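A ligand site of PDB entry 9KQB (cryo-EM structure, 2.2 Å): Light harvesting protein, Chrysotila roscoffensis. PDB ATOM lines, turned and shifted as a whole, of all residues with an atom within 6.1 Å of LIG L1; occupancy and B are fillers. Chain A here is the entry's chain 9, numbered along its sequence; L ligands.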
ATOM      1  N   TYR A  71      13.290   0.771  -7.337  1.00  0.00           N
ATOM      2  CA  TYR A  71      12.912   1.963  -8.089  1.00  0.00           C
ATOM      3  C   TYR A  71      11.537   2.464  -7.653  1.00  0.00           C
ATOM      4  O   TYR A  71      11.288   3.680  -7.614  1.00  0.00           O
ATOM      5  CB  TYR A  71      12.932   1.676  -9.589  1.00  0.00           C
ATOM      6  CG  TYR A  71      12.802   2.915 -10.443  1.00  0.00           C
ATOM      7  CD1 TYR A  71      13.469   4.084 -10.115  1.00  0.00           C
ATOM      8  CD2 TYR A  71      12.012   2.903 -11.584  1.00  0.00           C
ATOM      9  CE1 TYR A  71      13.349   5.217 -10.894  1.00  0.00           C
ATOM     10  CE2 TYR A  71      11.892   4.037 -12.376  1.00  0.00           C
ATOM     11  CZ  TYR A  71      12.563   5.188 -12.021  1.00  0.00           C
ATOM     12  OH  TYR A  71      12.439   6.314 -12.807  1.00  0.00           O
ATOM     13  N   PHE A  74      12.074   4.311  -4.493  1.00  0.00           N
ATOM     14  CA  PHE A  74      12.794   5.558  -4.731  1.00  0.00           C
ATOM     15  C   PHE A  74      11.908   6.588  -5.436  1.00  0.00           C
ATOM     16  O   PHE A  74      12.076   7.794  -5.213  1.00  0.00           O
ATOM     17  CB  PHE A  74      14.049   5.302  -5.555  1.00  0.00           C
ATOM     18  CG  PHE A  74      15.194   4.728  -4.759  1.00  0.00           C
ATOM     19  CD1 PHE A  74      15.311   4.988  -3.404  1.00  0.00           C
ATOM     20  CD2 PHE A  74      16.156   3.949  -5.379  1.00  0.00           C
ATOM     21  CE1 PHE A  74      16.369   4.469  -2.675  1.00  0.00           C
ATOM     22  CE2 PHE A  74      17.212   3.424  -4.658  1.00  0.00           C
ATOM     23  CZ  PHE A  74      17.319   3.687  -3.302  1.00  0.00           C
ATOM     24  N   GLN A  75      10.995   6.132  -6.288  1.00  0.00           N
ATOM     25  CA  GLN A  75      10.121   7.041  -7.017  1.00  0.00           C
ATOM     26  C   GLN A  75       9.185   7.788  -6.073  1.00  0.00           C
ATOM     27  O   GLN A  75       9.070   9.015  -6.128  1.00  0.00           O
ATOM     28  CB  GLN A  75       9.318   6.276  -8.062  1.00  0.00           C
ATOM     29  CG  GLN A  75      10.001   6.118  -9.406  1.00  0.00           C
ATOM     30  CD  GLN A  75       9.375   5.024 -10.249  1.00  0.00           C
ATOM     31  OE1 GLN A  75       9.382   3.855  -9.865  1.00  0.00           O
ATOM     32  NE2 GLN A  75       8.821   5.396 -11.392  1.00  0.00           N
ATOM     33  N   MET A  77       9.641   8.016  -2.920  1.00  0.00           N
ATOM     34  CA  MET A  77      10.474   8.707  -1.949  1.00  0.00           C
ATOM     35  C   MET A  77      10.846  10.097  -2.446  1.00  0.00           C
ATOM     36  O   MET A  77      10.825  11.068  -1.688  1.00  0.00           O
ATOM     37  CB  MET A  77      11.732   7.875  -1.669  1.00  0.00           C
ATOM     38  CG  MET A  77      12.238   7.923  -0.261  1.00  0.00           C
ATOM     39  SD  MET A  77      12.809   6.271   0.159  1.00  0.00           S
ATOM     40  CE  MET A  77      13.655   6.561   1.702  1.00  0.00           C
ATOM     41  N   GLU A  78      11.168  10.207  -3.736  1.00  0.00           N
ATOM     42  CA  GLU A  78      11.633  11.463  -4.295  1.00  0.00           C
ATOM     43  C   GLU A  78      10.506  12.482  -4.403  1.00  0.00           C
ATOM     44  O   GLU A  78      10.696  13.661  -4.096  1.00  0.00           O
ATOM     45  CB  GLU A  78      12.266  11.220  -5.669  1.00  0.00           C
ATOM     46  CG  GLU A  78      13.081  12.376  -6.200  1.00  0.00           C
ATOM     47  CD  GLU A  78      13.713  12.079  -7.539  1.00  0.00           C
ATOM     48  OE1 GLU A  78      13.117  11.295  -8.319  1.00  0.00           O
ATOM     49  OE2 GLU A  78      14.806  12.612  -7.820  1.00  0.00           O
ATOM     50  N   HIS A  81       9.341  13.465  -0.670  1.00  0.00           N
ATOM     51  CA  HIS A  81      10.362  14.302  -0.044  1.00  0.00           C
ATOM     52  C   HIS A  81      10.358  15.690  -0.663  1.00  0.00           C
ATOM     53  O   HIS A  81      10.517  16.700   0.029  1.00  0.00           O
ATOM     54  CB  HIS A  81      11.756  13.680  -0.186  1.00  0.00           C
ATOM     55  CG  HIS A  81      12.166  12.831   0.976  1.00  0.00           C
ATOM     56  ND1 HIS A  81      11.949  11.472   1.020  1.00  0.00           N
ATOM     57  CD2 HIS A  81      12.803  13.141   2.126  1.00  0.00           C
ATOM     58  CE1 HIS A  81      12.430  10.986   2.154  1.00  0.00           C
ATOM     59  NE2 HIS A  81      12.956  11.987   2.841  1.00  0.00           N
ATOM     60  N   ARG A 183       8.315  17.183 -10.501  1.00  0.00           N
ATOM     61  CA  ARG A 183       9.501  16.450 -10.055  1.00  0.00           C
ATOM     62  C   ARG A 183      10.742  17.332 -10.118  1.00  0.00           C
ATOM     63  O   ARG A 183      11.583  17.301  -9.212  1.00  0.00           O
ATOM     64  CB  ARG A 183       9.678  15.194 -10.907  1.00  0.00           C
ATOM     65  CG  ARG A 183      10.895  14.363 -10.527  1.00  0.00           C
ATOM     66  CD  ARG A 183      10.659  13.604  -9.232  1.00  0.00           C
ATOM     67  NE  ARG A 183       9.604  12.612  -9.373  1.00  0.00           N
ATOM     68  CZ  ARG A 183       9.776  11.399  -9.898  1.00  0.00           C
ATOM     69  NH1 ARG A 183      10.955  11.000 -10.329  1.00  0.00           N
ATOM     70  NH2 ARG A 183       8.736  10.585  -9.978  1.00  0.00           N
ATOM     71  N   GLY A 186      10.461  19.905  -7.452  1.00  0.00           N
ATOM     72  CA  GLY A 186      10.674  19.272  -6.161  1.00  0.00           C
ATOM     73  C   GLY A 186      12.153  19.061  -5.864  1.00  0.00           C
ATOM     74  O   GLY A 186      12.567  19.115  -4.702  1.00  0.00           O
ATOM     75  N   ARG A 187      12.952  18.801  -6.901  1.00  0.00           N
ATOM     76  CA  ARG A 187      14.385  18.620  -6.722  1.00  0.00           C
ATOM     77  C   ARG A 187      15.051  19.928  -6.307  1.00  0.00           C
ATOM     78  O   ARG A 187      15.983  19.935  -5.487  1.00  0.00           O
ATOM     79  CB  ARG A 187      15.010  18.078  -7.996  1.00  0.00           C
ATOM     80  CG  ARG A 187      14.722  16.600  -8.238  1.00  0.00           C
ATOM     81  CD  ARG A 187      14.832  16.242  -9.712  1.00  0.00           C
ATOM     82  NE  ARG A 187      14.329  14.899  -9.968  1.00  0.00           N
ATOM     83  CZ  ARG A 187      14.516  14.223 -11.097  1.00  0.00           C
ATOM     84  NH1 ARG A 187      15.212  14.743 -12.107  1.00  0.00           N
ATOM     85  NH2 ARG A 187      14.000  13.015 -11.229  1.00  0.00           N
ATOM     86  N   ALA A 188      14.581  21.049  -6.861  1.00  0.00           N
ATOM     87  CA  ALA A 188      15.132  22.346  -6.487  1.00  0.00           C
ATOM     88  C   ALA A 188      14.691  22.751  -5.084  1.00  0.00           C
ATOM     89  O   ALA A 188      15.472  23.337  -4.319  1.00  0.00           O
ATOM     90  CB  ALA A 188      14.711  23.407  -7.496  1.00  0.00           C
ATOM     91  N   MET A 190      13.958  20.778  -2.613  1.00  0.00           N
ATOM     92  CA  MET A 190      14.678  19.927  -1.675  1.00  0.00           C
ATOM     93  C   MET A 190      16.093  20.441  -1.431  1.00  0.00           C
ATOM     94  O   MET A 190      16.559  20.488  -0.284  1.00  0.00           O
ATOM     95  CB  MET A 190      14.653  18.492  -2.202  1.00  0.00           C
ATOM     96  CG  MET A 190      15.619  17.453  -1.633  1.00  0.00           C
ATOM     97  SD  MET A 190      15.922  17.244   0.126  1.00  0.00           S
ATOM     98  CE  MET A 190      17.691  17.559   0.120  1.00  0.00           C
ATOM     99  N   MET A 191      16.790  20.868  -2.486  1.00  0.00           N
ATOM    100  CA  MET A 191      18.137  21.407  -2.332  1.00  0.00           C
ATOM    101  C   MET A 191      18.136  22.717  -1.546  1.00  0.00           C
ATOM    102  O   MET A 191      19.052  22.988  -0.754  1.00  0.00           O
ATOM    103  CB  MET A 191      18.787  21.620  -3.696  1.00  0.00           C
ATOM    104  CG  MET A 191      20.292  21.364  -3.732  1.00  0.00           C
ATOM    105  SD  MET A 191      20.983  21.564  -5.394  1.00  0.00           S
ATOM    106  CE  MET A 191      20.876  23.339  -5.599  1.00  0.00           C
HETATM  107 MG1  LIG L   1      16.852  12.229  -7.578  1.00  0.00          MG
HETATM  108  C1  LIG L   1      17.156  10.516 -10.954  1.00  0.00           C
HETATM  109  C2  LIG L   1      15.913   9.225  -6.486  1.00  0.00           C
HETATM  110  C3  LIG L   1      16.883  13.842  -4.798  1.00  0.00           C
HETATM  111  C4  LIG L   1      18.250  15.196  -9.372  1.00  0.00           C
HETATM  112  N1  LIG L   1      16.549  10.144  -8.590  1.00  0.00           N
HETATM  113  C5  LIG L   1      16.674   9.728  -9.783  1.00  0.00           C
HETATM  114  C6  LIG L   1      16.254   8.293  -9.936  1.00  0.00           C
HETATM  115  C7  LIG L   1      15.584   8.011  -8.602  1.00  0.00           C
HETATM  116  C8  LIG L   1      16.029   9.194  -7.818  1.00  0.00           C
HETATM  117  C9  LIG L   1      14.068   8.004  -8.720  1.00  0.00           C
HETATM  118  C10 LIG L   1      17.443   7.361 -10.195  1.00  0.00           C
HETATM  119  C11 LIG L   1      18.740   7.781  -9.513  1.00  0.00           C
HETATM  120  C12 LIG L   1      18.897   7.095  -8.180  1.00  0.00           C
HETATM  121  O1  LIG L   1      18.329   6.044  -7.954  1.00  0.00           O
HETATM  122  O2  LIG L   1      19.725   7.694  -7.139  1.00  0.00           O
HETATM  123  N2  LIG L   1      16.469  11.592  -5.995  1.00  0.00           N
HETATM  124  C13 LIG L   1      16.086  10.378  -5.564  1.00  0.00           C
HETATM  125  C14 LIG L   1      15.845  10.292  -4.105  1.00  0.00           C
HETATM  126  C15 LIG L   1      16.147  11.667  -3.668  1.00  0.00           C
HETATM  127  C16 LIG L   1      16.517  12.405  -4.916  1.00  0.00           C
HETATM  128  C17 LIG L   1      15.415   9.101  -3.298  1.00  0.00           C
HETATM  129  C18 LIG L   1      16.135  12.356  -2.358  1.00  0.00           C
HETATM  130  C19 LIG L   1      15.154  12.165  -1.505  1.00  0.00           C
HETATM  131  N3  LIG L   1      17.490  14.213  -7.147  1.00  0.00           N
HETATM  132  C20 LIG L   1      17.385  14.696  -5.897  1.00  0.00           C
HETATM  133  C21 LIG L   1      17.818  16.112  -5.772  1.00  0.00           C
HETATM  134  C22 LIG L   1      18.211  16.462  -7.150  1.00  0.00           C
HETATM  135  C23 LIG L   1      17.964  15.207  -7.924  1.00  0.00           C
HETATM  136  C24 LIG L   1      17.854  16.989  -4.564  1.00  0.00           C
HETATM  137  C25 LIG L   1      18.729  17.787  -7.637  1.00  0.00           C
HETATM  138  C26 LIG L   1      20.227  17.745  -7.789  1.00  0.00           C
HETATM  139  N4  LIG L   1      17.602  12.858  -9.656  1.00  0.00           N
HETATM  140  C27 LIG L   1      18.058  13.995 -10.203  1.00  0.00           C
HETATM  141  C28 LIG L   1      18.322  13.885 -11.652  1.00  0.00           C
HETATM  142  C29 LIG L   1      17.947  12.485 -11.926  1.00  0.00           C
HETATM  143  C30 LIG L   1      17.536  11.929 -10.708  1.00  0.00           C
HETATM  144  C31 LIG L   1      18.828  14.937 -12.606  1.00  0.00           C
HETATM  145  C32 LIG L   1      17.854  11.445 -12.995  1.00  0.00           C
HETATM  146  O3  LIG L   1      18.148  11.590 -14.234  1.00  0.00           O
HETATM  147  C33 LIG L   1      17.103  10.307 -12.408  1.00  0.00           C
HETATM  148  C34 LIG L   1      15.677  10.350 -12.873  1.00  0.00           C
HETATM  149  O4  LIG L   1      15.008  11.346 -12.648  1.00  0.00           O
HETATM  150  O5  LIG L   1      14.979   9.109 -13.166  1.00  0.00           O
HETATM  151  C35 LIG L   1      15.695   7.988 -13.676  1.00  0.00           C
HETATM  152  C36 LIG L   1      19.520   7.323  -5.779  1.00  0.00           C
HETATM  153  C37 LIG L   1      20.573   7.972  -4.918  1.00  0.00           C
HETATM  154  C38 LIG L   1      20.474   8.018  -3.579  1.00  0.00           C
HETATM  155  C39 LIG L   1      19.287   7.419  -2.880  1.00  0.00           C
HETATM  156  C40 LIG L   1      21.565   8.682  -2.774  1.00  0.00           C
HETATM  157  C41 LIG L   1      20.947   9.519  -1.663  1.00  0.00           C
HETATM  158  C42 LIG L   1      21.762  10.778  -1.393  1.00  0.00           C
HETATM  159  C43 LIG L   1      22.953  10.499  -0.484  1.00  0.00           C
HETATM  160  C44 LIG L   1      22.513   9.800   0.801  1.00  0.00           C
HETATM  161  C45 LIG L   1      23.646  11.827  -0.182  1.00  0.00           C
HETATM  162  C46 LIG L   1      24.779  11.658   0.836  1.00  0.00           C
HETATM  163 MG1  LG2 L   2      14.365  12.032   4.114  1.00  0.00          MG
HETATM  164  C1  LG2 L   2      13.983   9.042   5.799  1.00  0.00           C
HETATM  165  C2  LG2 L   2      11.950  13.290   6.352  1.00  0.00           C
HETATM  166  C3  LG2 L   2      16.200  15.255   4.717  1.00  0.00           C
HETATM  167  C4  LG2 L   2      16.413  11.175   1.926  1.00  0.00           C
HETATM  168  N1  LG2 L   2      12.951  11.230   5.865  1.00  0.00           N
HETATM  169  C5  LG2 L   2      13.314  10.186   6.479  1.00  0.00           C
HETATM  170  C6  LG2 L   2      12.992  10.236   7.950  1.00  0.00           C
HETATM  171  C7  LG2 L   2      12.089  11.454   8.034  1.00  0.00           C
HETATM  172  C8  LG2 L   2      12.304  12.045   6.686  1.00  0.00           C
HETATM  173  C9  LG2 L   2      10.629  11.084   8.240  1.00  0.00           C
HETATM  174  C10 LG2 L   2      14.169  10.419   8.919  1.00  0.00           C
HETATM  175  C11 LG2 L   2      15.584  10.560   8.334  1.00  0.00           C
HETATM  176  C12 LG2 L   2      15.855  11.926   7.745  1.00  0.00           C
HETATM  177  O1  LG2 L   2      15.121  12.873   7.983  1.00  0.00           O
HETATM  178  O2  LG2 L   2      17.018  12.105   6.896  1.00  0.00           O
HETATM  179  N2  LG2 L   2      14.077  14.003   5.387  1.00  0.00           N
HETATM  180  C13 LG2 L   2      13.024  14.294   6.181  1.00  0.00           C
HETATM  181  C14 LG2 L   2      13.085  15.634   6.791  1.00  0.00           C
HETATM  182  C15 LG2 L   2      14.364  16.159   6.259  1.00  0.00           C
HETATM  183  C16 LG2 L   2      14.900  15.069   5.405  1.00  0.00           C
HETATM  184  C17 LG2 L   2      12.100  16.295   7.720  1.00  0.00           C
HETATM  185  C18 LG2 L   2      15.115  17.425   6.425  1.00  0.00           C
HETATM  186  C19 LG2 L   2      15.977  17.561   7.412  1.00  0.00           C
HETATM  187  N3  LG2 L   2      16.081  13.154   3.476  1.00  0.00           N
HETATM  188  C20 LG2 L   2      16.698  14.316   3.676  1.00  0.00           C
HETATM  189  C21 LG2 L   2      17.868  14.539   2.800  1.00  0.00           C
HETATM  190  C22 LG2 L   2      17.901  13.300   1.979  1.00  0.00           C
HETATM  191  C23 LG2 L   2      16.717  12.525   2.468  1.00  0.00           C
HETATM  192  C24 LG2 L   2      18.731  15.773   2.822  1.00  0.00           C
HETATM  193  C25 LG2 L   2      18.828  12.892   0.852  1.00  0.00           C
HETATM  194  C26 LG2 L   2      20.290  13.012   1.185  1.00  0.00           C
HETATM  195  N4  LG2 L   2      15.112  10.568   3.878  1.00  0.00           N
HETATM  196  C27 LG2 L   2      15.903  10.164   2.887  1.00  0.00           C
HETATM  197  C28 LG2 L   2      16.143   8.704   2.886  1.00  0.00           C
HETATM  198  C29 LG2 L   2      15.366   8.263   4.083  1.00  0.00           C
HETATM  199  C30 LG2 L   2      14.785   9.417   4.607  1.00  0.00           C
HETATM  200  C31 LG2 L   2      16.972   7.888   1.934  1.00  0.00           C
HETATM  201  C32 LG2 L   2      14.964   7.083   4.912  1.00  0.00           C
HETATM  202  O3  LG2 L   2      15.307   5.867   4.723  1.00  0.00           O
HETATM  203  C33 LG2 L   2      14.097   7.581   6.005  1.00  0.00           C
HETATM  204  C34 LG2 L   2      12.737   6.963   5.871  1.00  0.00           C
HETATM  205  O4  LG2 L   2      12.088   7.112   4.851  1.00  0.00           O
HETATM  206  O5  LG2 L   2      12.047   6.446   7.044  1.00  0.00           O
HETATM  207  C35 LG2 L   2      12.744   6.195   8.258  1.00  0.00           C
HETATM  208  C36 LG2 L   2      17.538  10.973   6.212  1.00  0.00           C
HETATM  209  C37 LG2 L   2      18.723  11.329   5.324  1.00  0.00           C
HETATM  210  C38 LG2 L   2      19.548  10.375   4.886  1.00  0.00           C
HETATM  211  C39 LG2 L   2      19.332   8.926   5.260  1.00  0.00           C
HETATM  212  C40 LG2 L   2      20.729  10.724   4.005  1.00  0.00           C
HETATM  213  C41 LG2 L   2      21.542  11.832   4.647  1.00  0.00           C
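The side-chain carboxylate (OE2) of Glu 78 is bound to a magnesium atom (MG1) of LIG L1 (2.1 Å).
The guanidinium group (NH2) of Arg 187 lies within hydrogen-bond range of an oxygen (O4) of LIG L1, at 2.4 Å.
A ring nitrogen (NE2) of His 81 binds a magnesium atom (MG1) of LG2 L2, 1.9 Å away.
OE1 of Glu 78 lies within salt-bridge range of NH2 of Arg 187.
The side-chain carboxylate of Glu 78 lies within salt-bridge range of the guanidinium group of Arg 183, at 3.0 Å.
The side-chain amide oxygen (OE1) of Gln 75 lies close to the backbone carbonyl oxygen (O) of Tyr 71, 3.0 Å away.
A ring nitrogen (ND1) of His 81 lies within hydrogen-bond range of the backbone carbonyl oxygen of Met 77, at 3.0 Å.
Merely in contact with LIG L1: Tyr 71 (3.6 Å), Met 190 (3.7 Å), His 81 (3.9 Å) and Phe 74 (3.97 Å).
Hydrophobic or aromatic side chains within 4 Å of LIG L1: Tyr 71, Phe 74, His 81 and Met 190.
Of the 12 residues printed, 6 come within 4 Å of LIG L1.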
